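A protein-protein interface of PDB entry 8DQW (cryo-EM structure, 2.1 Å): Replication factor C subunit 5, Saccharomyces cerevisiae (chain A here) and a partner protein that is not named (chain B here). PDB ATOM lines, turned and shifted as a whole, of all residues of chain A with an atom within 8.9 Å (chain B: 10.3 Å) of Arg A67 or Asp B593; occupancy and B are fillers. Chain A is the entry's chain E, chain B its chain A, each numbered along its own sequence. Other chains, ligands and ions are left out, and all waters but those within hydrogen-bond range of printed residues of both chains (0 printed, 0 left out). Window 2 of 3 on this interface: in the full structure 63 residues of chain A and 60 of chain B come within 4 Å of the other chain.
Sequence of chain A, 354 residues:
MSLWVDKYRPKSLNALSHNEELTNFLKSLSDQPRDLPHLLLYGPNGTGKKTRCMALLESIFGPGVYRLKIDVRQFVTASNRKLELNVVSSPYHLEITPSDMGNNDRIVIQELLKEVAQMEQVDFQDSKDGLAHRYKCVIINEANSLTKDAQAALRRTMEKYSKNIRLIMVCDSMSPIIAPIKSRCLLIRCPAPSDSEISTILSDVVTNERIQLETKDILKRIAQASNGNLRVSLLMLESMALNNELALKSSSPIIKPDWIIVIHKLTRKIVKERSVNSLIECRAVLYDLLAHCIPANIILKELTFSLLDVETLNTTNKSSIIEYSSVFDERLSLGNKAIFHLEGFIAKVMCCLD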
ATOM      1  N   LYS A  11       4.155 -34.147 -12.638  1.00  0.00           N
ATOM      2  CA  LYS A  11       4.951 -33.748 -11.481  1.00  0.00           C
ATOM      3  C   LYS A  11       4.854 -34.753 -10.337  1.00  0.00           C
ATOM      4  O   LYS A  11       5.138 -34.405  -9.186  1.00  0.00           O
ATOM      5  CB  LYS A  11       4.524 -32.359 -11.002  1.00  0.00           C
ATOM      6  CG  LYS A  11       4.823 -31.246 -11.999  1.00  0.00           C
ATOM      7  CD  LYS A  11       5.713 -30.164 -11.403  1.00  0.00           C
ATOM      8  CE  LYS A  11       6.630 -29.559 -12.454  1.00  0.00           C
ATOM      9  NZ  LYS A  11       7.013 -28.160 -12.116  1.00  0.00           N
ATOM     10  N   MET A  54      12.592 -37.094 -11.853  1.00  0.00           N
ATOM     11  CA  MET A  54      12.046 -36.024 -11.025  1.00  0.00           C
ATOM     12  C   MET A  54      10.833 -36.503 -10.237  1.00  0.00           C
ATOM     13  O   MET A  54      10.643 -36.106  -9.083  1.00  0.00           O
ATOM     14  CB  MET A  54      11.689 -34.817 -11.891  1.00  0.00           C
ATOM     15  CG  MET A  54      12.899 -34.032 -12.387  1.00  0.00           C
ATOM     16  SD  MET A  54      13.973 -33.439 -11.062  1.00  0.00           S
ATOM     17  CE  MET A  54      12.870 -32.312 -10.210  1.00  0.00           C
ATOM     18  N   GLY A  62       9.483 -34.529  -1.952  1.00  0.00           N
ATOM     19  CA  GLY A  62       8.293 -33.716  -2.032  1.00  0.00           C
ATOM     20  C   GLY A  62       8.320 -32.781  -3.225  1.00  0.00           C
ATOM     21  O   GLY A  62       9.266 -32.778  -4.019  1.00  0.00           O
ATOM     22  N   PRO A  63       7.274 -31.964  -3.376  1.00  0.00           N
ATOM     23  CA  PRO A  63       7.207 -31.065  -4.542  1.00  0.00           C
ATOM     24  C   PRO A  63       8.348 -30.065  -4.609  1.00  0.00           C
ATOM     25  O   PRO A  63       8.663 -29.581  -5.704  1.00  0.00           O
ATOM     26  CB  PRO A  63       5.855 -30.356  -4.367  1.00  0.00           C
ATOM     27  CG  PRO A  63       5.080 -31.205  -3.409  1.00  0.00           C
ATOM     28  CD  PRO A  63       6.088 -31.842  -2.511  1.00  0.00           C
ATOM     29  N   GLY A  64       8.986 -29.751  -3.481  1.00  0.00           N
ATOM     30  CA  GLY A  64      10.055 -28.769  -3.479  1.00  0.00           C
ATOM     31  C   GLY A  64      11.200 -29.109  -4.408  1.00  0.00           C
ATOM     32  O   GLY A  64      12.004 -28.230  -4.734  1.00  0.00           O
ATOM     33  N   VAL A  65      11.296 -30.366  -4.846  1.00  0.00           N
ATOM     34  CA  VAL A  65      12.349 -30.753  -5.774  1.00  0.00           C
ATOM     35  C   VAL A  65      12.225 -30.008  -7.093  1.00  0.00           C
ATOM     36  O   VAL A  65      13.196 -29.931  -7.853  1.00  0.00           O
ATOM     37  CB  VAL A  65      12.338 -32.280  -6.003  1.00  0.00           C
ATOM     38  CG1 VAL A  65      12.459 -33.024  -4.676  1.00  0.00           C
ATOM     39  CG2 VAL A  65      11.079 -32.706  -6.749  1.00  0.00           C
ATOM     40  N   TYR A  66      11.052 -29.451  -7.391  1.00  0.00           N
ATOM     41  CA  TYR A  66      10.842 -28.713  -8.628  1.00  0.00           C
ATOM     42  C   TYR A  66      11.175 -27.231  -8.501  1.00  0.00           C
ATOM     43  O   TYR A  66      11.069 -26.502  -9.493  1.00  0.00           O
ATOM     44  CB  TYR A  66       9.394 -28.886  -9.097  1.00  0.00           C
ATOM     45  CG  TYR A  66       9.070 -30.302  -9.517  1.00  0.00           C
ATOM     46  CD1 TYR A  66       9.547 -30.819 -10.715  1.00  0.00           C
ATOM     47  CD2 TYR A  66       8.300 -31.127  -8.708  1.00  0.00           C
ATOM     48  CE1 TYR A  66       9.257 -32.113 -11.100  1.00  0.00           C
ATOM     49  CE2 TYR A  66       8.006 -32.423  -9.085  1.00  0.00           C
ATOM     50  CZ  TYR A  66       8.487 -32.911 -10.281  1.00  0.00           C
ATOM     51  OH  TYR A  66       8.198 -34.201 -10.659  1.00  0.00           O
ATOM     52  N   ARG A  67      11.576 -26.772  -7.316  1.00  0.00           N
ATOM     53  CA  ARG A  67      11.989 -25.383  -7.107  1.00  0.00           C
ATOM     54  C   ARG A  67      13.479 -25.297  -7.412  1.00  0.00           C
ATOM     55  O   ARG A  67      14.324 -25.362  -6.518  1.00  0.00           O
ATOM     56  CB  ARG A  67      11.680 -24.938  -5.684  1.00  0.00           C
ATOM     57  CG  ARG A  67      10.199 -24.733  -5.401  1.00  0.00           C
ATOM     58  CD  ARG A  67       9.987 -23.802  -4.218  1.00  0.00           C
ATOM     59  NE  ARG A  67      10.422 -24.408  -2.964  1.00  0.00           N
ATOM     60  CZ  ARG A  67       9.741 -25.331  -2.300  1.00  0.00           C
ATOM     61  NH1 ARG A  67       8.574 -25.779  -2.736  1.00  0.00           N
ATOM     62  NH2 ARG A  67      10.244 -25.821  -1.170  1.00  0.00           N
ATOM     63  N   LEU A  68      13.803 -25.134  -8.689  1.00  0.00           N
ATOM     64  CA  LEU A  68      15.176 -25.216  -9.166  1.00  0.00           C
ATOM     65  C   LEU A  68      15.764 -23.824  -9.353  1.00  0.00           C
ATOM     66  O   LEU A  68      15.061 -22.888  -9.745  1.00  0.00           O
ATOM     67  CB  LEU A  68      15.243 -25.980 -10.491  1.00  0.00           C
ATOM     68  CG  LEU A  68      14.581 -27.359 -10.506  1.00  0.00           C
ATOM     69  CD1 LEU A  68      14.548 -27.918 -11.918  1.00  0.00           C
ATOM     70  CD2 LEU A  68      15.303 -28.310  -9.568  1.00  0.00           C
ATOM     71  N   LYS A  69      17.057 -23.696  -9.062  1.00  0.00           N
ATOM     72  CA  LYS A  69      17.808 -22.492  -9.387  1.00  0.00           C
ATOM     73  C   LYS A  69      19.150 -22.911  -9.968  1.00  0.00           C
ATOM     74  O   LYS A  69      19.520 -24.087  -9.945  1.00  0.00           O
ATOM     75  CB  LYS A  69      17.994 -21.582  -8.166  1.00  0.00           C
ATOM     76  CG  LYS A  69      18.396 -22.297  -6.892  1.00  0.00           C
ATOM     77  CD  LYS A  69      18.997 -21.314  -5.899  1.00  0.00           C
ATOM     78  CE  LYS A  69      20.445 -20.991  -6.232  1.00  0.00           C
ATOM     79  NZ  LYS A  69      20.808 -19.601  -5.837  1.00  0.00           N
ATOM     80  N   ILE A  70      19.882 -21.936 -10.500  1.00  0.00           N
ATOM     81  CA  ILE A  70      21.107 -22.187 -11.247  1.00  0.00           C
ATOM     82  C   ILE A  70      22.257 -21.441 -10.583  1.00  0.00           C
ATOM     83  O   ILE A  70      22.089 -20.309 -10.118  1.00  0.00           O
ATOM     84  CB  ILE A  70      20.962 -21.767 -12.725  1.00  0.00           C
ATOM     85  CG1 ILE A  70      22.187 -22.199 -13.536  1.00  0.00           C
ATOM     86  CG2 ILE A  70      20.762 -20.261 -12.840  1.00  0.00           C
ATOM     87  CD1 ILE A  70      22.260 -23.685 -13.788  1.00  0.00           C
ATOM     88  N   VAL A  88      22.565 -26.978 -11.510  1.00  0.00           N
ATOM     89  CA  VAL A  88      21.180 -26.749 -11.121  1.00  0.00           C
ATOM     90  C   VAL A  88      20.973 -27.359  -9.745  1.00  0.00           C
ATOM     91  O   VAL A  88      21.533 -28.413  -9.435  1.00  0.00           O
ATOM     92  CB  VAL A  88      20.208 -27.341 -12.161  1.00  0.00           C
ATOM     93  CG1 VAL A  88      18.844 -27.610 -11.539  1.00  0.00           C
ATOM     94  CG2 VAL A  88      20.081 -26.407 -13.351  1.00  0.00           C
ATOM     95  N   SER A  89      20.187 -26.696  -8.905  1.00  0.00           N
ATOM     96  CA  SER A  89      20.029 -27.138  -7.529  1.00  0.00           C
ATOM     97  C   SER A  89      18.595 -26.942  -7.064  1.00  0.00           C
ATOM     98  O   SER A  89      17.939 -25.958  -7.418  1.00  0.00           O
ATOM     99  CB  SER A  89      20.985 -26.386  -6.594  1.00  0.00           C
ATOM    100  OG  SER A  89      20.895 -24.985  -6.789  1.00  0.00           O
ATOM    101  N   SER A  90      18.127 -27.900  -6.277  1.00  0.00           N
ATOM    102  CA  SER A  90      16.914 -27.820  -5.483  1.00  0.00           C
ATOM    103  C   SER A  90      17.292 -28.177  -4.056  1.00  0.00           C
ATOM    104  O   SER A  90      18.281 -28.884  -3.828  1.00  0.00           O
ATOM    105  CB  SER A  90      15.831 -28.779  -5.994  1.00  0.00           C
ATOM    106  OG  SER A  90      15.788 -29.956  -5.205  1.00  0.00           O
ATOM    107  N   PRO A  91      16.512 -27.734  -3.072  1.00  0.00           N
ATOM    108  CA  PRO A  91      16.919 -27.924  -1.670  1.00  0.00           C
ATOM    109  C   PRO A  91      17.241 -29.367  -1.304  1.00  0.00           C
ATOM    110  O   PRO A  91      17.778 -29.620  -0.221  1.00  0.00           O
ATOM    111  CB  PRO A  91      15.711 -27.406  -0.875  1.00  0.00           C
ATOM    112  CG  PRO A  91      14.583 -27.324  -1.849  1.00  0.00           C
ATOM    113  CD  PRO A  91      15.189 -27.097  -3.189  1.00  0.00           C
ATOM    114  N   TYR A  92      16.929 -30.322  -2.185  1.00  0.00           N
ATOM    115  CA  TYR A  92      17.175 -31.727  -1.910  1.00  0.00           C
ATOM    116  C   TYR A  92      18.097 -32.421  -2.904  1.00  0.00           C
ATOM    117  O   TYR A  92      18.520 -33.549  -2.628  1.00  0.00           O
ATOM    118  CB  TYR A  92      15.848 -32.499  -1.862  1.00  0.00           C
ATOM    119  CG  TYR A  92      14.752 -31.786  -1.105  1.00  0.00           C
ATOM    120  CD1 TYR A  92      13.782 -31.055  -1.778  1.00  0.00           C
ATOM    121  CD2 TYR A  92      14.689 -31.841   0.281  1.00  0.00           C
ATOM    122  CE1 TYR A  92      12.777 -30.402  -1.091  1.00  0.00           C
ATOM    123  CE2 TYR A  92      13.687 -31.190   0.976  1.00  0.00           C
ATOM    124  CZ  TYR A  92      12.736 -30.472   0.286  1.00  0.00           C
ATOM    125  OH  TYR A  92      11.737 -29.821   0.972  1.00  0.00           O
ATOM    126  N   HIS A  93      18.427 -31.804  -4.037  1.00  0.00           N
ATOM    127  CA  HIS A  93      19.207 -32.515  -5.043  1.00  0.00           C
ATOM    128  C   HIS A  93      19.949 -31.526  -5.933  1.00  0.00           C
ATOM    129  O   HIS A  93      19.687 -30.321  -5.926  1.00  0.00           O
ATOM    130  CB  HIS A  93      18.316 -33.438  -5.887  1.00  0.00           C
ATOM    131  CG  HIS A  93      17.687 -32.762  -7.065  1.00  0.00           C
ATOM    132  ND1 HIS A  93      16.544 -31.999  -6.964  1.00  0.00           N
ATOM    133  CD2 HIS A  93      18.044 -32.735  -8.370  1.00  0.00           C
ATOM    134  CE1 HIS A  93      16.223 -31.531  -8.157  1.00  0.00           C
ATOM    135  NE2 HIS A  93      17.117 -31.964  -9.028  1.00  0.00           N
ATOM    136  N   GLU A  95      21.858 -31.162 -10.047  1.00  0.00           N
ATOM    137  CA  GLU A  95      21.837 -31.611 -11.433  1.00  0.00           C
ATOM    138  C   GLU A  95      23.045 -31.023 -12.145  1.00  0.00           C
ATOM    139  O   GLU A  95      23.262 -29.806 -12.092  1.00  0.00           O
ATOM    140  CB  GLU A  95      20.548 -31.174 -12.143  1.00  0.00           C
ATOM    141  CG  GLU A  95      19.302 -31.922 -11.719  1.00  0.00           C
ATOM    142  CD  GLU A  95      18.051 -31.395 -12.401  1.00  0.00           C
ATOM    143  OE1 GLU A  95      18.077 -31.217 -13.637  1.00  0.00           O
ATOM    144  OE2 GLU A  95      17.043 -31.158 -11.701  1.00  0.00           O
ATOM    145  N   LEU B 468      15.330 -20.636 -18.560  1.00  0.00           N
ATOM    146  CA  LEU B 468      15.414 -20.865 -17.122  1.00  0.00           C
ATOM    147  C   LEU B 468      14.806 -19.710 -16.339  1.00  0.00           C
ATOM    148  O   LEU B 468      14.104 -19.929 -15.345  1.00  0.00           O
ATOM    149  CB  LEU B 468      16.871 -21.076 -16.706  1.00  0.00           C
ATOM    150  CG  LEU B 468      17.371 -22.522 -16.682  1.00  0.00           C
ATOM    151  CD1 LEU B 468      18.876 -22.559 -16.469  1.00  0.00           C
ATOM    152  CD2 LEU B 468      16.658 -23.320 -15.601  1.00  0.00           C
ATOM    153  N   TYR B 471      10.636 -19.363 -17.528  1.00  0.00           N
ATOM    154  CA  TYR B 471       9.689 -20.470 -17.496  1.00  0.00           C
ATOM    155  C   TYR B 471      10.071 -21.581 -16.528  1.00  0.00           C
ATOM    156  O   TYR B 471       9.380 -22.604 -16.495  1.00  0.00           O
ATOM    157  CB  TYR B 471       9.527 -21.058 -18.907  1.00  0.00           C
ATOM    158  CG  TYR B 471       9.144 -20.028 -19.945  1.00  0.00           C
ATOM    159  CD1 TYR B 471       7.826 -19.617 -20.091  1.00  0.00           C
ATOM    160  CD2 TYR B 471      10.103 -19.456 -20.770  1.00  0.00           C
ATOM    161  CE1 TYR B 471       7.472 -18.671 -21.036  1.00  0.00           C
ATOM    162  CE2 TYR B 471       9.759 -18.509 -21.717  1.00  0.00           C
ATOM    163  CZ  TYR B 471       8.442 -18.121 -21.845  1.00  0.00           C
ATOM    164  OH  TYR B 471       8.095 -17.180 -22.787  1.00  0.00           O
ATOM    165  N   ASN B 472      11.133 -21.418 -15.739  1.00  0.00           N
ATOM    166  CA  ASN B 472      11.551 -22.433 -14.774  1.00  0.00           C
ATOM    167  C   ASN B 472      11.718 -23.790 -15.453  1.00  0.00           C
ATOM    168  O   ASN B 472      11.342 -24.835 -14.915  1.00  0.00           O
ATOM    169  CB  ASN B 472      10.560 -22.519 -13.610  1.00  0.00           C
ATOM    170  CG  ASN B 472      11.025 -23.459 -12.513  1.00  0.00           C
ATOM    171  OD1 ASN B 472      10.325 -24.405 -12.152  1.00  0.00           O
ATOM    172  ND2 ASN B 472      12.212 -23.200 -11.976  1.00  0.00           N
ATOM    173  N   ALA B 473      12.288 -23.772 -16.655  1.00  0.00           N
ATOM    174  CA  ALA B 473      12.536 -24.978 -17.434  1.00  0.00           C
ATOM    175  C   ALA B 473      14.029 -25.095 -17.702  1.00  0.00           C
ATOM    176  O   ALA B 473      14.668 -24.120 -18.111  1.00  0.00           O
ATOM    177  CB  ALA B 473      11.758 -24.953 -18.752  1.00  0.00           C
ATOM    178  N   VAL B 474      14.577 -26.284 -17.469  1.00  0.00           N
ATOM    179  CA  VAL B 474      15.984 -26.578 -17.716  1.00  0.00           C
ATOM    180  C   VAL B 474      16.059 -27.596 -18.845  1.00  0.00           C
ATOM    181  O   VAL B 474      15.429 -28.658 -18.775  1.00  0.00           O
ATOM    182  CB  VAL B 474      16.689 -27.097 -16.450  1.00  0.00           C
ATOM    183  CG1 VAL B 474      15.912 -28.249 -15.820  1.00  0.00           C
ATOM    184  CG2 VAL B 474      18.116 -27.521 -16.771  1.00  0.00           C
ATOM    185  N   TYR B 584      13.611 -11.681 -12.209  1.00  0.00           N
ATOM    186  CA  TYR B 584      13.401 -12.808 -11.307  1.00  0.00           C
ATOM    187  C   TYR B 584      13.623 -12.440  -9.844  1.00  0.00           C
ATOM    188  O   TYR B 584      13.051 -13.083  -8.958  1.00  0.00           O
ATOM    189  CB  TYR B 584      14.329 -13.961 -11.699  1.00  0.00           C
ATOM    190  CG  TYR B 584      14.350 -15.104 -10.708  1.00  0.00           C
ATOM    191  CD1 TYR B 584      13.204 -15.843 -10.446  1.00  0.00           C
ATOM    192  CD2 TYR B 584      15.517 -15.445 -10.038  1.00  0.00           C
ATOM    193  CE1 TYR B 584      13.220 -16.888  -9.542  1.00  0.00           C
ATOM    194  CE2 TYR B 584      15.542 -16.489  -9.133  1.00  0.00           C
ATOM    195  CZ  TYR B 584      14.392 -17.207  -8.889  1.00  0.00           C
ATOM    196  OH  TYR B 584      14.413 -18.246  -7.989  1.00  0.00           O
ATOM    197  N   ASN B 587      10.497 -11.573  -7.801  1.00  0.00           N
ATOM    198  CA  ASN B 587       9.468 -12.603  -7.705  1.00  0.00           C
ATOM    199  C   ASN B 587       9.490 -13.284  -6.341  1.00  0.00           C
ATOM    200  O   ASN B 587       8.435 -13.553  -5.756  1.00  0.00           O
ATOM    201  CB  ASN B 587       9.653 -13.633  -8.819  1.00  0.00           C
ATOM    202  CG  ASN B 587       9.381 -13.058 -10.195  1.00  0.00           C
ATOM    203  OD1 ASN B 587       8.774 -11.995 -10.326  1.00  0.00           O
ATOM    204  ND2 ASN B 587       9.828 -13.759 -11.228  1.00  0.00           N
ATOM    205  N   VAL B 588      10.685 -13.572  -5.819  1.00  0.00           N
ATOM    206  CA  VAL B 588      10.786 -14.278  -4.543  1.00  0.00           C
ATOM    207  C   VAL B 588      10.178 -13.441  -3.424  1.00  0.00           C
ATOM    208  O   VAL B 588       9.410 -13.942  -2.595  1.00  0.00           O
ATOM    209  CB  VAL B 588      12.253 -14.636  -4.244  1.00  0.00           C
ATOM    210  CG1 VAL B 588      12.352 -15.450  -2.961  1.00  0.00           C
ATOM    211  CG2 VAL B 588      12.866 -15.399  -5.412  1.00  0.00           C
ATOM    212  N   MET B 589      10.513 -12.148  -3.383  1.00  0.00           N
ATOM    213  CA  MET B 589      10.004 -11.292  -2.317  1.00  0.00           C
ATOM    214  C   MET B 589       8.534 -10.947  -2.525  1.00  0.00           C
ATOM    215  O   MET B 589       7.821 -10.680  -1.551  1.00  0.00           O
ATOM    216  CB  MET B 589      10.837 -10.013  -2.226  1.00  0.00           C
ATOM    217  CG  MET B 589      11.939 -10.057  -1.175  1.00  0.00           C
ATOM    218  SD  MET B 589      12.179  -8.472  -0.350  1.00  0.00           S
ATOM    219  CE  MET B 589      11.041  -8.631   1.025  1.00  0.00           C
ATOM    220  N   MET B 590       8.066 -10.944  -3.774  1.00  0.00           N
ATOM    221  CA  MET B 590       6.673 -10.600  -4.040  1.00  0.00           C
ATOM    222  C   MET B 590       5.730 -11.582  -3.357  1.00  0.00           C
ATOM    223  O   MET B 590       4.763 -11.178  -2.701  1.00  0.00           O
ATOM    224  CB  MET B 590       6.433 -10.565  -5.553  1.00  0.00           C
ATOM    225  CG  MET B 590       5.017 -10.935  -6.004  1.00  0.00           C
ATOM    226  SD  MET B 590       3.732  -9.773  -5.489  1.00  0.00           S
ATOM    227  CE  MET B 590       4.545  -8.191  -5.700  1.00  0.00           C
ATOM    228  N   ALA B 591       6.000 -12.877  -3.496  1.00  0.00           N
ATOM    229  CA  ALA B 591       5.177 -13.910  -2.883  1.00  0.00           C
ATOM    230  C   ALA B 591       5.829 -15.260  -3.143  1.00  0.00           C
ATOM    231  O   ALA B 591       6.605 -15.421  -4.090  1.00  0.00           O
ATOM    232  CB  ALA B 591       3.744 -13.899  -3.427  1.00  0.00           C
ATOM    233  N   ASN B 592       5.503 -16.227  -2.289  1.00  0.00           N
ATOM    234  CA  ASN B 592       5.975 -17.595  -2.429  1.00  0.00           C
ATOM    235  C   ASN B 592       4.802 -18.548  -2.258  1.00  0.00           C
ATOM    236  O   ASN B 592       3.859 -18.268  -1.513  1.00  0.00           O
ATOM    237  CB  ASN B 592       7.070 -17.923  -1.404  1.00  0.00           C
ATOM    238  CG  ASN B 592       8.431 -17.393  -1.814  1.00  0.00           C
ATOM    239  OD1 ASN B 592       8.761 -17.345  -3.000  1.00  0.00           O
ATOM    240  ND2 ASN B 592       9.231 -16.992  -0.832  1.00  0.00           N
ATOM    241  N   ASP B 593       4.868 -19.682  -2.959  1.00  0.00           N
ATOM    242  CA  ASP B 593       3.778 -20.650  -2.888  1.00  0.00           C
ATOM    243  C   ASP B 593       3.618 -21.193  -1.473  1.00  0.00           C
ATOM    244  O   ASP B 593       2.494 -21.324  -0.976  1.00  0.00           O
ATOM    245  CB  ASP B 593       4.019 -21.784  -3.887  1.00  0.00           C
ATOM    246  CG  ASP B 593       4.976 -22.837  -3.364  1.00  0.00           C
ATOM    247  OD1 ASP B 593       4.527 -23.735  -2.621  1.00  0.00           O
ATOM    248  OD2 ASP B 593       6.178 -22.767  -3.696  1.00  0.00           O
ATOM    249  N   ASP B 594       4.732 -21.499  -0.805  1.00  0.00           N
ATOM    250  CA  ASP B 594       4.705 -22.013   0.561  1.00  0.00           C
ATOM    251  C   ASP B 594       3.685 -23.141   0.689  1.00  0.00           C
ATOM    252  O   ASP B 594       3.790 -24.155  -0.008  1.00  0.00           O
ATOM    253  CB  ASP B 594       4.402 -20.878   1.543  1.00  0.00           C
ATOM    254  CG  ASP B 594       5.470 -19.802   1.535  1.00  0.00           C
ATOM    255  OD1 ASP B 594       6.589 -20.076   1.054  1.00  0.00           O
ATOM    256  OD2 ASP B 594       5.190 -18.681   2.009  1.00  0.00           O
ATOM    257  N   LEU B 595       2.699 -22.982   1.572  1.00  0.00           N
ATOM    258  CA  LEU B 595       1.644 -23.965   1.773  1.00  0.00           C
ATOM    259  C   LEU B 595       0.306 -23.242   1.863  1.00  0.00           C
ATOM    260  O   LEU B 595       0.235 -22.010   1.821  1.00  0.00           O
ATOM    261  CB  LEU B 595       1.900 -24.805   3.031  1.00  0.00           C
ATOM    262  CG  LEU B 595       3.250 -25.520   3.093  1.00  0.00           C
ATOM    263  CD1 LEU B 595       3.525 -26.025   4.500  1.00  0.00           C
ATOM    264  CD2 LEU B 595       3.299 -26.663   2.091  1.00  0.00           C
ATOM    265  N   GLU B 596      -0.766 -24.020   1.989  1.00  0.00           N
ATOM    266  CA  GLU B 596      -2.112 -23.475   2.089  1.00  0.00           C
ATOM    267  C   GLU B 596      -2.424 -23.145   3.542  1.00  0.00           C
ATOM    268  O   GLU B 596      -2.304 -24.005   4.421  1.00  0.00           O
ATOM    269  CB  GLU B 596      -3.138 -24.467   1.538  1.00  0.00           C
ATOM    270  CG  GLU B 596      -2.848 -24.931   0.118  1.00  0.00           C
ATOM    271  CD  GLU B 596      -3.878 -25.919  -0.394  1.00  0.00           C
ATOM    272  OE1 GLU B 596      -3.699 -27.135  -0.170  1.00  0.00           O
ATOM    273  OE2 GLU B 596      -4.865 -25.480  -1.021  1.00  0.00           O
ATOM    274  N   ASP B 597      -2.822 -21.897   3.790  1.00  0.00           N
ATOM    275  CA  ASP B 597      -3.128 -21.444   5.142  1.00  0.00           C
ATOM    276  C   ASP B 597      -4.449 -20.686   5.170  1.00  0.00           C
ATOM    277  O   ASP B 597      -5.149 -20.607   4.155  1.00  0.00           O
ATOM    278  CB  ASP B 597      -1.999 -20.561   5.677  1.00  0.00           C
ATOM    279  CG  ASP B 597      -0.627 -21.166   5.449  1.00  0.00           C
ATOM    280  OD1 ASP B 597      -0.290 -22.154   6.135  1.00  0.00           O
ATOM    281  OD2 ASP B 597       0.113 -20.654   4.583  1.00  0.00           O
ATOM    282  N   GLU B 599      -5.787 -17.685   4.802  1.00  0.00           N
ATOM    283  CA  GLU B 599      -5.597 -16.325   4.309  1.00  0.00           C
ATOM    284  C   GLU B 599      -6.774 -15.429   4.669  1.00  0.00           C
ATOM    285  O   GLU B 599      -6.589 -14.234   4.926  1.00  0.00           O
ATOM    286  CB  GLU B 599      -5.384 -16.341   2.796  1.00  0.00           C
ATOM    287  CG  GLU B 599      -4.086 -17.006   2.365  1.00  0.00           C
ATOM    288  CD  GLU B 599      -3.934 -17.068   0.858  1.00  0.00           C
ATOM    289  OE1 GLU B 599      -4.922 -16.791   0.147  1.00  0.00           O
ATOM    290  OE2 GLU B 599      -2.825 -17.394   0.386  1.00  0.00           O
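Among the printed residues, pairs that only touch across the chains: Leu A68 with Asn B472 (3.6 Å).
Of the printed residues of chain B, Tyr A66 touches Asn B472 (3.5 Å).
Leu A68 touches just one residue of chain B: Asn B472.
Of the printed residues of chain A, Asn B472 touches Tyr A66 (3.5 Å) and Leu A68 (3.6 Å).
Met B589 touches none of the printed residues of chain A.
Asp B593 touches just one residue of chain A: Arg A67.
No residue of chain A comes within 4 Å of Asp B594.
The nearest residue of chain A that does not touch Asp B593 is Pro A63 (7.0 Å).
The backbone carbonyl oxygen (O) of Tyr A66 lies close to the side-chain amide oxygen (OD1) of Asn B472, 3.5 Å away.
The guanidinium group (NH1) of Arg A67 is in salt-bridge range of the side-chain carboxylate (OD2) of Asp B593.
O of Lys A11 lies close to OH of Tyr A66, at 3.4 Å.
The backbone carbonyl oxygen of Met A54 sits at hydrogen-bond distance from the side-chain hydroxyl of Tyr A66 (3.5 Å).
Of the 18 printed residues of chain A, 3 touch a printed residue of chain B.
Among the printed residues, Asp or Glu carboxylates within 4 Å of a Lys or Arg side-chain nitrogen of the other chain: Arg A67 with Asp B593.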
